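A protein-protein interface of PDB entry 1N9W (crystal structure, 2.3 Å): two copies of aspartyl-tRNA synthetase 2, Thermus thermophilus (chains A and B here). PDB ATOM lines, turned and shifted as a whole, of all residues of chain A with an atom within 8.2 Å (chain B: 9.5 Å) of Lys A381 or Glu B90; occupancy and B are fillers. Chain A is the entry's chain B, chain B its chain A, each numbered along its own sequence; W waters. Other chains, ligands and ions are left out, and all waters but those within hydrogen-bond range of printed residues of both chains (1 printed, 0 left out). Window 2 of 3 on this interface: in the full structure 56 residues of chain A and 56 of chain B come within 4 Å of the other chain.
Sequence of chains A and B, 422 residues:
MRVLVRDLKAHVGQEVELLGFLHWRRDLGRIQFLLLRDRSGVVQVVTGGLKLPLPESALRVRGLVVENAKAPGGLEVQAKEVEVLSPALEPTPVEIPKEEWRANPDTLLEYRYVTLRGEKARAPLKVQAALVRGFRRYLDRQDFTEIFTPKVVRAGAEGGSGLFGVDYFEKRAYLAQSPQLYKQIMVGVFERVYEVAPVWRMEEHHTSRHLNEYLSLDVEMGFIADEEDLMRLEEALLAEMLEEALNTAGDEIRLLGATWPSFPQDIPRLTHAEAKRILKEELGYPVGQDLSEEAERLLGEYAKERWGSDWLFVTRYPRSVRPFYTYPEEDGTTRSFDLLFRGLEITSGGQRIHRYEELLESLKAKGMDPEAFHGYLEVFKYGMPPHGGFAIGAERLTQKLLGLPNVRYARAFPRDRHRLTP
The side-chain hydroxyl (OG) of Ser B86 sits at hydrogen-bond distance from the backbone carbonyl oxygen (O) of Met A384 (2.8 Å).
The backbone NH of Leu B89 is in hydrogen-bond range of the backbone carbonyl oxygen of Lys A381 (3.3 Å).
The side-chain hydroxyl (OH) of Tyr A382 lies within hydrogen-bond range of the backbone carbonyl oxygen (O) of Pro B91 (3.2 Å).
OH of Tyr B113 lies within hydrogen-bond range of OE2 of Glu A378 (3.1 Å).
NH1 of Arg B117 sits at hydrogen-bond distance from O of Tyr A382 (2.9 Å).
The backbone carbonyl oxygen of Tyr A382 sits close to the backbone carbonyl oxygen of Glu B56 (3.1 Å).
The guanidinium group of Arg B117 is in salt-bridge range of the side-chain carboxylate of Glu B56 (3.2 Å).
The backbone carbonyl oxygen (O) of Ser B86 is in hydrogen-bond range of the backbone NH (N) of Ala B58 (3.1 Å).
N of Tyr B111 sits close to OH of Tyr B113, 3.4 Å away.
The side-chain carboxylate (OE1) of Glu A378 is in salt-bridge range of the side-chain amino group (NZ) of Lys A381 (3.1 Å).
Among the printed residues, pairs that only touch across the chains: Tyr A382 with Pro B93 (3.0 Å), Gly A383 with Ser B86 (3.2 Å), Tyr A382 with Tyr B113 (3.4 Å), Gly A383 with Ala B58 (3.5 Å), Lys A381 with Glu B90 (3.5 Å), Val A379 with Tyr B113 (3.6 Å), Tyr A382 with Thr B92 (3.6 Å), Tyr A356 with Leu B89 (3.6 Å), Gly A383 with Ala B88 (3.6 Å), Tyr A382 with Glu B90 (3.6 Å), Gly A383 with Glu B56 (3.7 Å) and Met A384 with Arg B117 (3.9 Å).
Tyr A376 touches none of the printed residues of chain B.
Of chain B, only Tyr B113 comes within 4 Å of Glu A378.
Of chain B, only Glu B56 (3.1 Å), Glu B90 (3.6 Å), Pro B91 (3.2 Å), Thr B92 (3.6 Å), Pro B93 (3.0 Å), Tyr B113 (3.4 Å) and Arg B117 (2.9 Å) come within 4 Å of Tyr A382.
Of the printed residues of chain A, Leu B89 touches Tyr A356 and Lys A381.
Of chain A, only Lys A381 and Tyr A382 come within 4 Å of Glu B90.
Of the printed residues of chain A, Arg B117 touches Tyr A382 and Met A384.
The nearest residue of chain B that does not touch Lys A381 is Ala B88 (4.1 Å).
The nearest residue of chain A that does not touch Glu B90 is Glu A378 (6.1 Å).
Of the 19 printed residues of chain B, 11 touch a printed residue of chain A.
Printed residues of chain B that touch a printed residue of chain A: Glu B56, Ala B58, Ser B86, Ala B88, Leu B89, Glu B90, Pro B91, Thr B92, Pro B93, Tyr B113 and Arg B117.
Among the printed residues, no Asp or Glu carboxylate lies within 4 Å of a Lys or Arg side-chain nitrogen of the other chain.
No position is printed for both chains.
Of the 18 pairs that touch across the chains among the printed residues, none has its exchanged pair printed and touching as well.
Water W1 lies within hydrogen-bond range of O of His A354 (2.5 Å), N of Met A384 (2.7 Å), O of Phe A380 (3.0 Å) and OG of Ser B86 (3.4 Å).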
ATOM      1  N   HIS A 354      -1.560   3.578  29.597  1.00  0.00           N
ATOM      2  CA  HIS A 354      -1.401   4.755  28.739  1.00  0.00           C
ATOM      3  C   HIS A 354      -0.206   5.638  29.062  1.00  0.00           C
ATOM      4  O   HIS A 354       0.244   6.406  28.212  1.00  0.00           O
ATOM      5  CB  HIS A 354      -2.664   5.609  28.780  1.00  0.00           C
ATOM      6  CG  HIS A 354      -3.097   5.978  30.163  1.00  0.00           C
ATOM      7  ND1 HIS A 354      -3.627   5.060  31.043  1.00  0.00           N
ATOM      8  CD2 HIS A 354      -3.099   7.167  30.810  1.00  0.00           C
ATOM      9  CE1 HIS A 354      -3.942   5.670  32.173  1.00  0.00           C
ATOM     10  NE2 HIS A 354      -3.632   6.946  32.058  1.00  0.00           N
ATOM     11  N   ARG A 355       0.299   5.545  30.285  1.00  0.00           N
ATOM     12  CA  ARG A 355       1.444   6.356  30.683  1.00  0.00           C
ATOM     13  C   ARG A 355       2.754   5.717  30.250  1.00  0.00           C
ATOM     14  O   ARG A 355       2.988   4.532  30.480  1.00  0.00           O
ATOM     15  CB  ARG A 355       1.442   6.568  32.200  1.00  0.00           C
ATOM     16  CG  ARG A 355       0.545   7.707  32.673  1.00  0.00           C
ATOM     17  CD  ARG A 355       1.223   9.078  32.553  1.00  0.00           C
ATOM     18  NE  ARG A 355       2.224   9.298  33.602  1.00  0.00           N
ATOM     19  CZ  ARG A 355       3.482   8.859  33.563  1.00  0.00           C
ATOM     20  NH1 ARG A 355       3.928   8.172  32.519  1.00  0.00           N
ATOM     21  NH2 ARG A 355       4.297   9.103  34.580  1.00  0.00           N
ATOM     22  N   TYR A 356       3.600   6.514  29.612  1.00  0.00           N
ATOM     23  CA  TYR A 356       4.891   6.041  29.142  1.00  0.00           C
ATOM     24  C   TYR A 356       5.690   5.435  30.286  1.00  0.00           C
ATOM     25  O   TYR A 356       6.189   4.315  30.184  1.00  0.00           O
ATOM     26  CB  TYR A 356       5.684   7.195  28.541  1.00  0.00           C
ATOM     27  CG  TYR A 356       7.075   6.812  28.107  1.00  0.00           C
ATOM     28  CD1 TYR A 356       7.280   6.043  26.965  1.00  0.00           C
ATOM     29  CD2 TYR A 356       8.191   7.228  28.833  1.00  0.00           C
ATOM     30  CE1 TYR A 356       8.563   5.704  26.549  1.00  0.00           C
ATOM     31  CE2 TYR A 356       9.478   6.893  28.426  1.00  0.00           C
ATOM     32  CZ  TYR A 356       9.656   6.135  27.285  1.00  0.00           C
ATOM     33  OH  TYR A 356      10.924   5.825  26.858  1.00  0.00           O
ATOM     34  N   GLU A 357       5.814   6.186  31.374  1.00  0.00           N
ATOM     35  CA  GLU A 357       6.555   5.709  32.531  1.00  0.00           C
ATOM     36  C   GLU A 357       6.064   4.353  33.015  1.00  0.00           C
ATOM     37  O   GLU A 357       6.865   3.475  33.318  1.00  0.00           O
ATOM     38  CB  GLU A 357       6.477   6.722  33.677  1.00  0.00           C
ATOM     39  CG  GLU A 357       7.382   7.926  33.486  1.00  0.00           C
ATOM     40  CD  GLU A 357       8.811   7.524  33.147  1.00  0.00           C
ATOM     41  OE1 GLU A 357       9.404   6.715  33.898  1.00  0.00           O
ATOM     42  OE2 GLU A 357       9.340   8.015  32.126  1.00  0.00           O
ATOM     43  N   LEU A 359       4.609   2.045  31.321  1.00  0.00           N
ATOM     44  CA  LEU A 359       4.937   1.005  30.352  1.00  0.00           C
ATOM     45  C   LEU A 359       6.360   0.494  30.556  1.00  0.00           C
ATOM     46  O   LEU A 359       6.597  -0.714  30.588  1.00  0.00           O
ATOM     47  CB  LEU A 359       4.797   1.529  28.919  1.00  0.00           C
ATOM     48  CG  LEU A 359       3.400   1.559  28.297  1.00  0.00           C
ATOM     49  CD1 LEU A 359       3.471   2.212  26.932  1.00  0.00           C
ATOM     50  CD2 LEU A 359       2.860   0.147  28.180  1.00  0.00           C
ATOM     51  N   LEU A 360       7.303   1.421  30.691  1.00  0.00           N
ATOM     52  CA  LEU A 360       8.703   1.065  30.884  1.00  0.00           C
ATOM     53  C   LEU A 360       8.894   0.121  32.062  1.00  0.00           C
ATOM     54  O   LEU A 360       9.574  -0.898  31.949  1.00  0.00           O
ATOM     55  CB  LEU A 360       9.550   2.317  31.111  1.00  0.00           C
ATOM     56  CG  LEU A 360       9.899   3.155  29.883  1.00  0.00           C
ATOM     57  CD1 LEU A 360      10.786   4.322  30.295  1.00  0.00           C
ATOM     58  CD2 LEU A 360      10.615   2.285  28.857  1.00  0.00           C
ATOM     59  N   HIS A 374      11.000   0.438  21.627  1.00  0.00           N
ATOM     60  CA  HIS A 374      11.137   1.877  21.452  1.00  0.00           C
ATOM     61  C   HIS A 374      10.133   2.416  20.434  1.00  0.00           C
ATOM     62  O   HIS A 374       9.554   3.482  20.632  1.00  0.00           O
ATOM     63  CB  HIS A 374      12.564   2.227  21.019  1.00  0.00           C
ATOM     64  CG  HIS A 374      12.808   3.698  20.874  1.00  0.00           C
ATOM     65  ND1 HIS A 374      12.275   4.444  19.843  1.00  0.00           N
ATOM     66  CD2 HIS A 374      13.514   4.564  21.639  1.00  0.00           C
ATOM     67  CE1 HIS A 374      12.642   5.706  19.981  1.00  0.00           C
ATOM     68  NE2 HIS A 374      13.395   5.806  21.063  1.00  0.00           N
ATOM     69  N   TYR A 376       7.329   1.203  19.830  1.00  0.00           N
ATOM     70  CA  TYR A 376       6.006   1.006  20.406  1.00  0.00           C
ATOM     71  C   TYR A 376       5.731   2.047  21.486  1.00  0.00           C
ATOM     72  O   TYR A 376       4.617   2.559  21.601  1.00  0.00           O
ATOM     73  CB  TYR A 376       5.915  -0.394  21.018  1.00  0.00           C
ATOM     74  CG  TYR A 376       4.630  -0.666  21.766  1.00  0.00           C
ATOM     75  CD1 TYR A 376       3.431  -0.846  21.084  1.00  0.00           C
ATOM     76  CD2 TYR A 376       4.611  -0.722  23.158  1.00  0.00           C
ATOM     77  CE1 TYR A 376       2.241  -1.079  21.773  1.00  0.00           C
ATOM     78  CE2 TYR A 376       3.428  -0.954  23.857  1.00  0.00           C
ATOM     79  CZ  TYR A 376       2.247  -1.130  23.160  1.00  0.00           C
ATOM     80  OH  TYR A 376       1.072  -1.347  23.846  1.00  0.00           O
ATOM     81  N   LEU A 377       6.760   2.352  22.269  1.00  0.00           N
ATOM     82  CA  LEU A 377       6.656   3.310  23.364  1.00  0.00           C
ATOM     83  C   LEU A 377       6.475   4.760  22.904  1.00  0.00           C
ATOM     84  O   LEU A 377       5.948   5.585  23.646  1.00  0.00           O
ATOM     85  CB  LEU A 377       7.901   3.203  24.257  1.00  0.00           C
ATOM     86  CG  LEU A 377       8.194   1.856  24.929  1.00  0.00           C
ATOM     87  CD1 LEU A 377       9.592   1.880  25.528  1.00  0.00           C
ATOM     88  CD2 LEU A 377       7.154   1.563  26.001  1.00  0.00           C
ATOM     89  N   GLU A 378       6.903   5.061  21.685  1.00  0.00           N
ATOM     90  CA  GLU A 378       6.805   6.411  21.147  1.00  0.00           C
ATOM     91  C   GLU A 378       5.469   7.118  21.312  1.00  0.00           C
ATOM     92  O   GLU A 378       5.388   8.154  21.975  1.00  0.00           O
ATOM     93  CB  GLU A 378       7.196   6.418  19.671  1.00  0.00           C
ATOM     94  CG  GLU A 378       8.679   6.603  19.463  1.00  0.00           C
ATOM     95  CD  GLU A 378       9.156   7.957  19.956  1.00  0.00           C
ATOM     96  OE1 GLU A 378      10.380   8.139  20.105  1.00  0.00           O
ATOM     97  OE2 GLU A 378       8.306   8.844  20.188  1.00  0.00           O
ATOM     98  N   VAL A 379       4.420   6.571  20.711  1.00  0.00           N
ATOM     99  CA  VAL A 379       3.108   7.198  20.801  1.00  0.00           C
ATOM    100  C   VAL A 379       2.695   7.509  22.238  1.00  0.00           C
ATOM    101  O   VAL A 379       2.089   8.546  22.497  1.00  0.00           O
ATOM    102  CB  VAL A 379       2.011   6.323  20.142  1.00  0.00           C
ATOM    103  CG1 VAL A 379       1.846   5.020  20.903  1.00  0.00           C
ATOM    104  CG2 VAL A 379       0.697   7.087  20.102  1.00  0.00           C
ATOM    105  N   PHE A 380       3.027   6.624  23.171  1.00  0.00           N
ATOM    106  CA  PHE A 380       2.646   6.846  24.560  1.00  0.00           C
ATOM    107  C   PHE A 380       3.376   8.018  25.217  1.00  0.00           C
ATOM    108  O   PHE A 380       3.290   8.221  26.427  1.00  0.00           O
ATOM    109  CB  PHE A 380       2.843   5.574  25.381  1.00  0.00           C
ATOM    110  CG  PHE A 380       2.002   4.424  24.913  1.00  0.00           C
ATOM    111  CD1 PHE A 380       2.448   3.591  23.889  1.00  0.00           C
ATOM    112  CD2 PHE A 380       0.754   4.179  25.482  1.00  0.00           C
ATOM    113  CE1 PHE A 380       1.665   2.533  23.442  1.00  0.00           C
ATOM    114  CE2 PHE A 380      -0.036   3.123  25.040  1.00  0.00           C
ATOM    115  CZ  PHE A 380       0.420   2.295  24.016  1.00  0.00           C
ATOM    116  N   LYS A 381       4.097   8.782  24.408  1.00  0.00           N
ATOM    117  CA  LYS A 381       4.806   9.954  24.889  1.00  0.00           C
ATOM    118  C   LYS A 381       4.037  11.177  24.398  1.00  0.00           C
ATOM    119  O   LYS A 381       4.557  12.293  24.373  1.00  0.00           O
ATOM    120  CB  LYS A 381       6.238   9.963  24.349  1.00  0.00           C
ATOM    121  CG  LYS A 381       7.175   9.052  25.125  1.00  0.00           C
ATOM    122  CD  LYS A 381       8.362   8.596  24.290  1.00  0.00           C
ATOM    123  CE  LYS A 381       8.937   9.673  23.498  1.00  0.00           C
ATOM    124  NZ  LYS A 381      10.094   9.578  22.834  1.00  0.00           N
ATOM    125  N   TYR A 382       2.787  10.951  23.998  1.00  0.00           N
ATOM    126  CA  TYR A 382       1.945  12.027  23.499  1.00  0.00           C
ATOM    127  C   TYR A 382       0.536  11.995  24.066  1.00  0.00           C
ATOM    128  O   TYR A 382      -0.449  11.949  23.329  1.00  0.00           O
ATOM    129  CB  TYR A 382       1.916  12.000  21.975  1.00  0.00           C
ATOM    130  CG  TYR A 382       3.271  12.282  21.369  1.00  0.00           C
ATOM    131  CD1 TYR A 382       3.755  13.587  21.271  1.00  0.00           C
ATOM    132  CD2 TYR A 382       4.093  11.238  20.934  1.00  0.00           C
ATOM    133  CE1 TYR A 382       5.025  13.847  20.754  1.00  0.00           C
ATOM    134  CE2 TYR A 382       5.363  11.486  20.418  1.00  0.00           C
ATOM    135  CZ  TYR A 382       5.822  12.794  20.332  1.00  0.00           C
ATOM    136  OH  TYR A 382       7.077  13.043  19.829  1.00  0.00           O
ATOM    137  N   GLY A 383       0.464  12.016  25.393  1.00  0.00           N
ATOM    138  CA  GLY A 383      -0.805  12.028  26.090  1.00  0.00           C
ATOM    139  C   GLY A 383      -1.855  11.021  25.669  1.00  0.00           C
ATOM    140  O   GLY A 383      -3.033  11.366  25.564  1.00  0.00           O
ATOM    141  N   MET A 384      -1.451   9.780  25.421  1.00  0.00           N
ATOM    142  CA  MET A 384      -2.421   8.758  25.058  1.00  0.00           C
ATOM    143  C   MET A 384      -3.352   8.692  26.268  1.00  0.00           C
ATOM    144  O   MET A 384      -2.906   8.452  27.391  1.00  0.00           O
ATOM    145  CB  MET A 384      -1.734   7.404  24.853  1.00  0.00           C
ATOM    146  CG  MET A 384      -2.602   6.389  24.132  1.00  0.00           C
ATOM    147  SD  MET A 384      -2.882   6.780  22.389  1.00  0.00           S
ATOM    148  CE  MET A 384      -2.016   5.488  21.680  1.00  0.00           C
ATOM    149  N   ARG B  25      -1.894  25.897  22.639  1.00  0.00           N
ATOM    150  CA  ARG B  25      -2.017  26.604  23.910  1.00  0.00           C
ATOM    151  C   ARG B  25      -1.161  27.863  23.933  1.00  0.00           C
ATOM    152  O   ARG B  25      -0.280  28.041  23.090  1.00  0.00           O
ATOM    153  CB  ARG B  25      -1.595  25.695  25.063  1.00  0.00           C
ATOM    154  CG  ARG B  25      -0.096  25.470  25.136  1.00  0.00           C
ATOM    155  CD  ARG B  25       0.208  24.099  25.706  1.00  0.00           C
ATOM    156  NE  ARG B  25       1.570  23.973  26.218  1.00  0.00           N
ATOM    157  CZ  ARG B  25       2.674  24.244  25.528  1.00  0.00           C
ATOM    158  NH1 ARG B  25       2.603  24.673  24.273  1.00  0.00           N
ATOM    159  NH2 ARG B  25       3.858  24.068  26.098  1.00  0.00           N
ATOM    160  N   PRO B  53      -0.043  22.106  30.116  1.00  0.00           N
ATOM    161  CA  PRO B  53       0.739  20.892  29.828  1.00  0.00           C
ATOM    162  C   PRO B  53       1.250  20.970  28.391  1.00  0.00           C
ATOM    163  O   PRO B  53       0.837  21.847  27.640  1.00  0.00           O
ATOM    164  CB  PRO B  53      -0.280  19.766  30.000  1.00  0.00           C
ATOM    165  CG  PRO B  53      -1.357  20.367  30.856  1.00  0.00           C
ATOM    166  CD  PRO B  53      -1.460  21.771  30.321  1.00  0.00           C
ATOM    167  N   LEU B  54       2.135  20.062  27.996  1.00  0.00           N
ATOM    168  CA  LEU B  54       2.631  20.108  26.628  1.00  0.00           C
ATOM    169  C   LEU B  54       1.493  19.796  25.655  1.00  0.00           C
ATOM    170  O   LEU B  54       0.490  19.175  26.033  1.00  0.00           O
ATOM    171  CB  LEU B  54       3.786  19.117  26.418  1.00  0.00           C
ATOM    172  CG  LEU B  54       5.183  19.488  26.948  1.00  0.00           C
ATOM    173  CD1 LEU B  54       5.576  20.887  26.441  1.00  0.00           C
ATOM    174  CD2 LEU B  54       5.187  19.452  28.469  1.00  0.00           C
ATOM    175  N   PRO B  55       1.619  20.253  24.395  1.00  0.00           N
ATOM    176  CA  PRO B  55       0.588  20.002  23.387  1.00  0.00           C
ATOM    177  C   PRO B  55       0.356  18.506  23.227  1.00  0.00           C
ATOM    178  O   PRO B  55       1.242  17.699  23.516  1.00  0.00           O
ATOM    179  CB  PRO B  55       1.177  20.624  22.126  1.00  0.00           C
ATOM    180  CG  PRO B  55       1.969  21.769  22.665  1.00  0.00           C
ATOM    181  CD  PRO B  55       2.652  21.163  23.873  1.00  0.00           C
ATOM    182  N   GLU B  56      -0.842  18.143  22.779  1.00  0.00           N
ATOM    183  CA  GLU B  56      -1.206  16.746  22.558  1.00  0.00           C
ATOM    184  C   GLU B  56      -1.563  15.997  23.832  1.00  0.00           C
ATOM    185  O   GLU B  56      -1.704  14.772  23.824  1.00  0.00           O
ATOM    186  CB  GLU B  56      -0.080  16.032  21.805  1.00  0.00           C
ATOM    187  CG  GLU B  56      -0.571  15.245  20.626  1.00  0.00           C
ATOM    188  CD  GLU B  56      -1.701  15.950  19.890  1.00  0.00           C
ATOM    189  OE1 GLU B  56      -1.480  17.048  19.358  1.00  0.00           O
ATOM    190  OE2 GLU B  56      -2.822  15.407  19.875  1.00  0.00           O
ATOM    191  N   SER B  57      -1.696  16.737  24.931  1.00  0.00           N
ATOM    192  CA  SER B  57      -2.071  16.153  26.220  1.00  0.00           C
ATOM    193  C   SER B  57      -3.585  15.890  26.202  1.00  0.00           C
ATOM    194  O   SER B  57      -4.339  16.610  25.548  1.00  0.00           O
ATOM    195  CB  SER B  57      -1.742  17.127  27.366  1.00  0.00           C
ATOM    196  OG  SER B  57      -0.346  17.325  27.525  1.00  0.00           O
ATOM    197  N   ALA B  58      -4.015  14.856  26.913  1.00  0.00           N
ATOM    198  CA  ALA B  58      -5.429  14.515  27.000  1.00  0.00           C
ATOM    199  C   ALA B  58      -6.008  15.289  28.173  1.00  0.00           C
ATOM    200  O   ALA B  58      -5.499  15.195  29.292  1.00  0.00           O
ATOM    201  CB  ALA B  58      -5.606  13.026  27.220  1.00  0.00           C
ATOM    202  N   SER B  86      -3.864  12.777  30.837  1.00  0.00           N
ATOM    203  CA  SER B  86      -2.637  12.135  30.415  1.00  0.00           C
ATOM    204  C   SER B  86      -1.689  13.168  29.831  1.00  0.00           C
ATOM    205  O   SER B  86      -1.852  13.610  28.694  1.00  0.00           O
ATOM    206  CB  SER B  86      -2.936  11.051  29.378  1.00  0.00           C
ATOM    207  OG  SER B  86      -1.743  10.533  28.825  1.00  0.00           O
ATOM    208  N   PRO B  87      -0.688  13.577  30.623  1.00  0.00           N
ATOM    209  CA  PRO B  87       0.324  14.561  30.240  1.00  0.00           C
ATOM    210  C   PRO B  87       1.252  14.053  29.143  1.00  0.00           C
ATOM    211  O   PRO B  87       1.733  12.920  29.196  1.00  0.00           O
ATOM    212  CB  PRO B  87       1.089  14.798  31.541  1.00  0.00           C
ATOM    213  CG  PRO B  87       0.100  14.456  32.602  1.00  0.00           C
ATOM    214  CD  PRO B  87      -0.548  13.225  32.046  1.00  0.00           C
ATOM    215  N   ALA B  88       1.498  14.899  28.152  1.00  0.00           N
ATOM    216  CA  ALA B  88       2.398  14.556  27.062  1.00  0.00           C
ATOM    217  C   ALA B  88       3.810  14.831  27.574  1.00  0.00           C
ATOM    218  O   ALA B  88       4.030  15.790  28.313  1.00  0.00           O
ATOM    219  CB  ALA B  88       2.098  15.416  25.836  1.00  0.00           C
ATOM    220  N   LEU B  89       4.767  13.994  27.192  1.00  0.00           N
ATOM    221  CA  LEU B  89       6.138  14.170  27.653  1.00  0.00           C
ATOM    222  C   LEU B  89       6.991  14.959  26.675  1.00  0.00           C
ATOM    223  O   LEU B  89       7.330  16.117  26.921  1.00  0.00           O
ATOM    224  CB  LEU B  89       6.785  12.815  27.917  1.00  0.00           C
ATOM    225  CG  LEU B  89       5.987  11.866  28.820  1.00  0.00           C
ATOM    226  CD1 LEU B  89       6.778  10.587  29.028  1.00  0.00           C
ATOM    227  CD2 LEU B  89       5.695  12.531  30.154  1.00  0.00           C
ATOM    228  N   GLU B  90       7.338  14.341  25.558  1.00  0.00           N
ATOM    229  CA  GLU B  90       8.168  15.012  24.572  1.00  0.00           C
ATOM    230  C   GLU B  90       7.371  15.975  23.702  1.00  0.00           C
ATOM    231  O   GLU B  90       6.148  15.849  23.576  1.00  0.00           O
ATOM    232  CB  GLU B  90       8.844  13.971  23.674  1.00  0.00           C
ATOM    233  CG  GLU B  90       9.714  12.980  24.422  1.00  0.00           C
ATOM    234  CD  GLU B  90      10.850  13.656  25.155  1.00  0.00           C
ATOM    235  OE1 GLU B  90      11.616  14.398  24.499  1.00  0.00           O
ATOM    236  OE2 GLU B  90      10.980  13.449  26.385  1.00  0.00           O
ATOM    237  N   PRO B  91       8.055  16.979  23.123  1.00  0.00           N
ATOM    238  CA  PRO B  91       7.369  17.939  22.256  1.00  0.00           C
ATOM    239  C   PRO B  91       7.002  17.131  21.019  1.00  0.00           C
ATOM    240  O   PRO B  91       7.543  16.044  20.817  1.00  0.00           O
ATOM    241  CB  PRO B  91       8.450  18.968  21.949  1.00  0.00           C
ATOM    242  CG  PRO B  91       9.318  18.921  23.154  1.00  0.00           C
ATOM    243  CD  PRO B  91       9.421  17.436  23.427  1.00  0.00           C
ATOM    244  N   THR B  92       6.092  17.639  20.200  1.00  0.00           N
ATOM    245  CA  THR B  92       5.692  16.908  19.004  1.00  0.00           C
ATOM    246  C   THR B  92       6.601  17.231  17.818  1.00  0.00           C
ATOM    247  O   THR B  92       6.897  18.396  17.550  1.00  0.00           O
ATOM    248  CB  THR B  92       4.248  17.239  18.602  1.00  0.00           C
ATOM    249  OG1 THR B  92       4.174  18.612  18.197  1.00  0.00           O
ATOM    250  CG2 THR B  92       3.306  17.006  19.778  1.00  0.00           C
ATOM    251  N   PRO B  93       7.053  16.196  17.088  1.00  0.00           N
ATOM    252  CA  PRO B  93       7.930  16.366  15.925  1.00  0.00           C
ATOM    253  C   PRO B  93       7.381  17.392  14.934  1.00  0.00           C
ATOM    254  O   PRO B  93       8.117  17.918  14.099  1.00  0.00           O
ATOM    255  CB  PRO B  93       7.984  14.963  15.335  1.00  0.00           C
ATOM    256  CG  PRO B  93       7.893  14.095  16.550  1.00  0.00           C
ATOM    257  CD  PRO B  93       6.788  14.768  17.338  1.00  0.00           C
ATOM    258  N   TYR B 111       5.810  10.849  14.620  1.00  0.00           N
ATOM    259  CA  TYR B 111       5.569  10.981  13.189  1.00  0.00           C
ATOM    260  C   TYR B 111       4.109  10.690  12.841  1.00  0.00           C
ATOM    261  O   TYR B 111       3.226  11.501  13.133  1.00  0.00           O
ATOM    262  CB  TYR B 111       6.501  10.043  12.409  1.00  0.00           C
ATOM    263  CG  TYR B 111       6.348  10.130  10.905  1.00  0.00           C
ATOM    264  CD1 TYR B 111       6.401  11.360  10.248  1.00  0.00           C
ATOM    265  CD2 TYR B 111       6.147   8.980  10.137  1.00  0.00           C
ATOM    266  CE1 TYR B 111       6.255  11.445   8.866  1.00  0.00           C
ATOM    267  CE2 TYR B 111       5.999   9.056   8.752  1.00  0.00           C
ATOM    268  CZ  TYR B 111       6.054  10.292   8.123  1.00  0.00           C
ATOM    269  OH  TYR B 111       5.904  10.375   6.757  1.00  0.00           O
ATOM    270  N   TYR B 113       2.140   8.162  14.009  1.00  0.00           N
ATOM    271  CA  TYR B 113       1.422   7.814  15.228  1.00  0.00           C
ATOM    272  C   TYR B 113       0.887   9.015  16.006  1.00  0.00           C
ATOM    273  O   TYR B 113       0.219   8.845  17.023  1.00  0.00           O
ATOM    274  CB  TYR B 113       2.328   6.974  16.131  1.00  0.00           C
ATOM    275  CG  TYR B 113       3.625   7.660  16.503  1.00  0.00           C
ATOM    276  CD1 TYR B 113       3.678   8.584  17.545  1.00  0.00           C
ATOM    277  CD2 TYR B 113       4.795   7.412  15.784  1.00  0.00           C
ATOM    278  CE1 TYR B 113       4.863   9.245  17.864  1.00  0.00           C
ATOM    279  CE2 TYR B 113       5.985   8.068  16.094  1.00  0.00           C
ATOM    280  CZ  TYR B 113       6.009   8.984  17.135  1.00  0.00           C
ATOM    281  OH  TYR B 113       7.179   9.641  17.434  1.00  0.00           O
ATOM    282  N   VAL B 114       1.176  10.224  15.530  1.00  0.00           N
ATOM    283  CA  VAL B 114       0.704  11.429  16.196  1.00  0.00           C
ATOM    284  C   VAL B 114       0.191  12.475  15.208  1.00  0.00           C
ATOM    285  O   VAL B 114      -0.752  13.213  15.505  1.00  0.00           O
ATOM    286  CB  VAL B 114       1.825  12.058  17.076  1.00  0.00           C
ATOM    287  CG1 VAL B 114       2.932  12.626  16.198  1.00  0.00           C
ATOM    288  CG2 VAL B 114       1.242  13.139  17.971  1.00  0.00           C
ATOM    289  N   ARG B 117      -3.546  12.588  14.036  1.00  0.00           N
ATOM    290  CA  ARG B 117      -4.523  13.200  14.929  1.00  0.00           C
ATOM    291  C   ARG B 117      -5.080  14.499  14.380  1.00  0.00           C
ATOM    292  O   ARG B 117      -6.163  14.927  14.770  1.00  0.00           O
ATOM    293  CB  ARG B 117      -3.893  13.473  16.297  1.00  0.00           C
ATOM    294  CG  ARG B 117      -3.488  12.233  17.051  1.00  0.00           C
ATOM    295  CD  ARG B 117      -2.956  12.596  18.419  1.00  0.00           C
ATOM    296  NE  ARG B 117      -2.540  11.414  19.167  1.00  0.00           N
ATOM    297  CZ  ARG B 117      -2.180  11.425  20.448  1.00  0.00           C
ATOM    298  NH1 ARG B 117      -2.183  12.560  21.135  1.00  0.00           N
ATOM    299  NH2 ARG B 117      -1.818  10.301  21.047  1.00  0.00           N
HETATM  300  O   HOH W   1       0.361   8.607  26.960  1.00  0.00           O
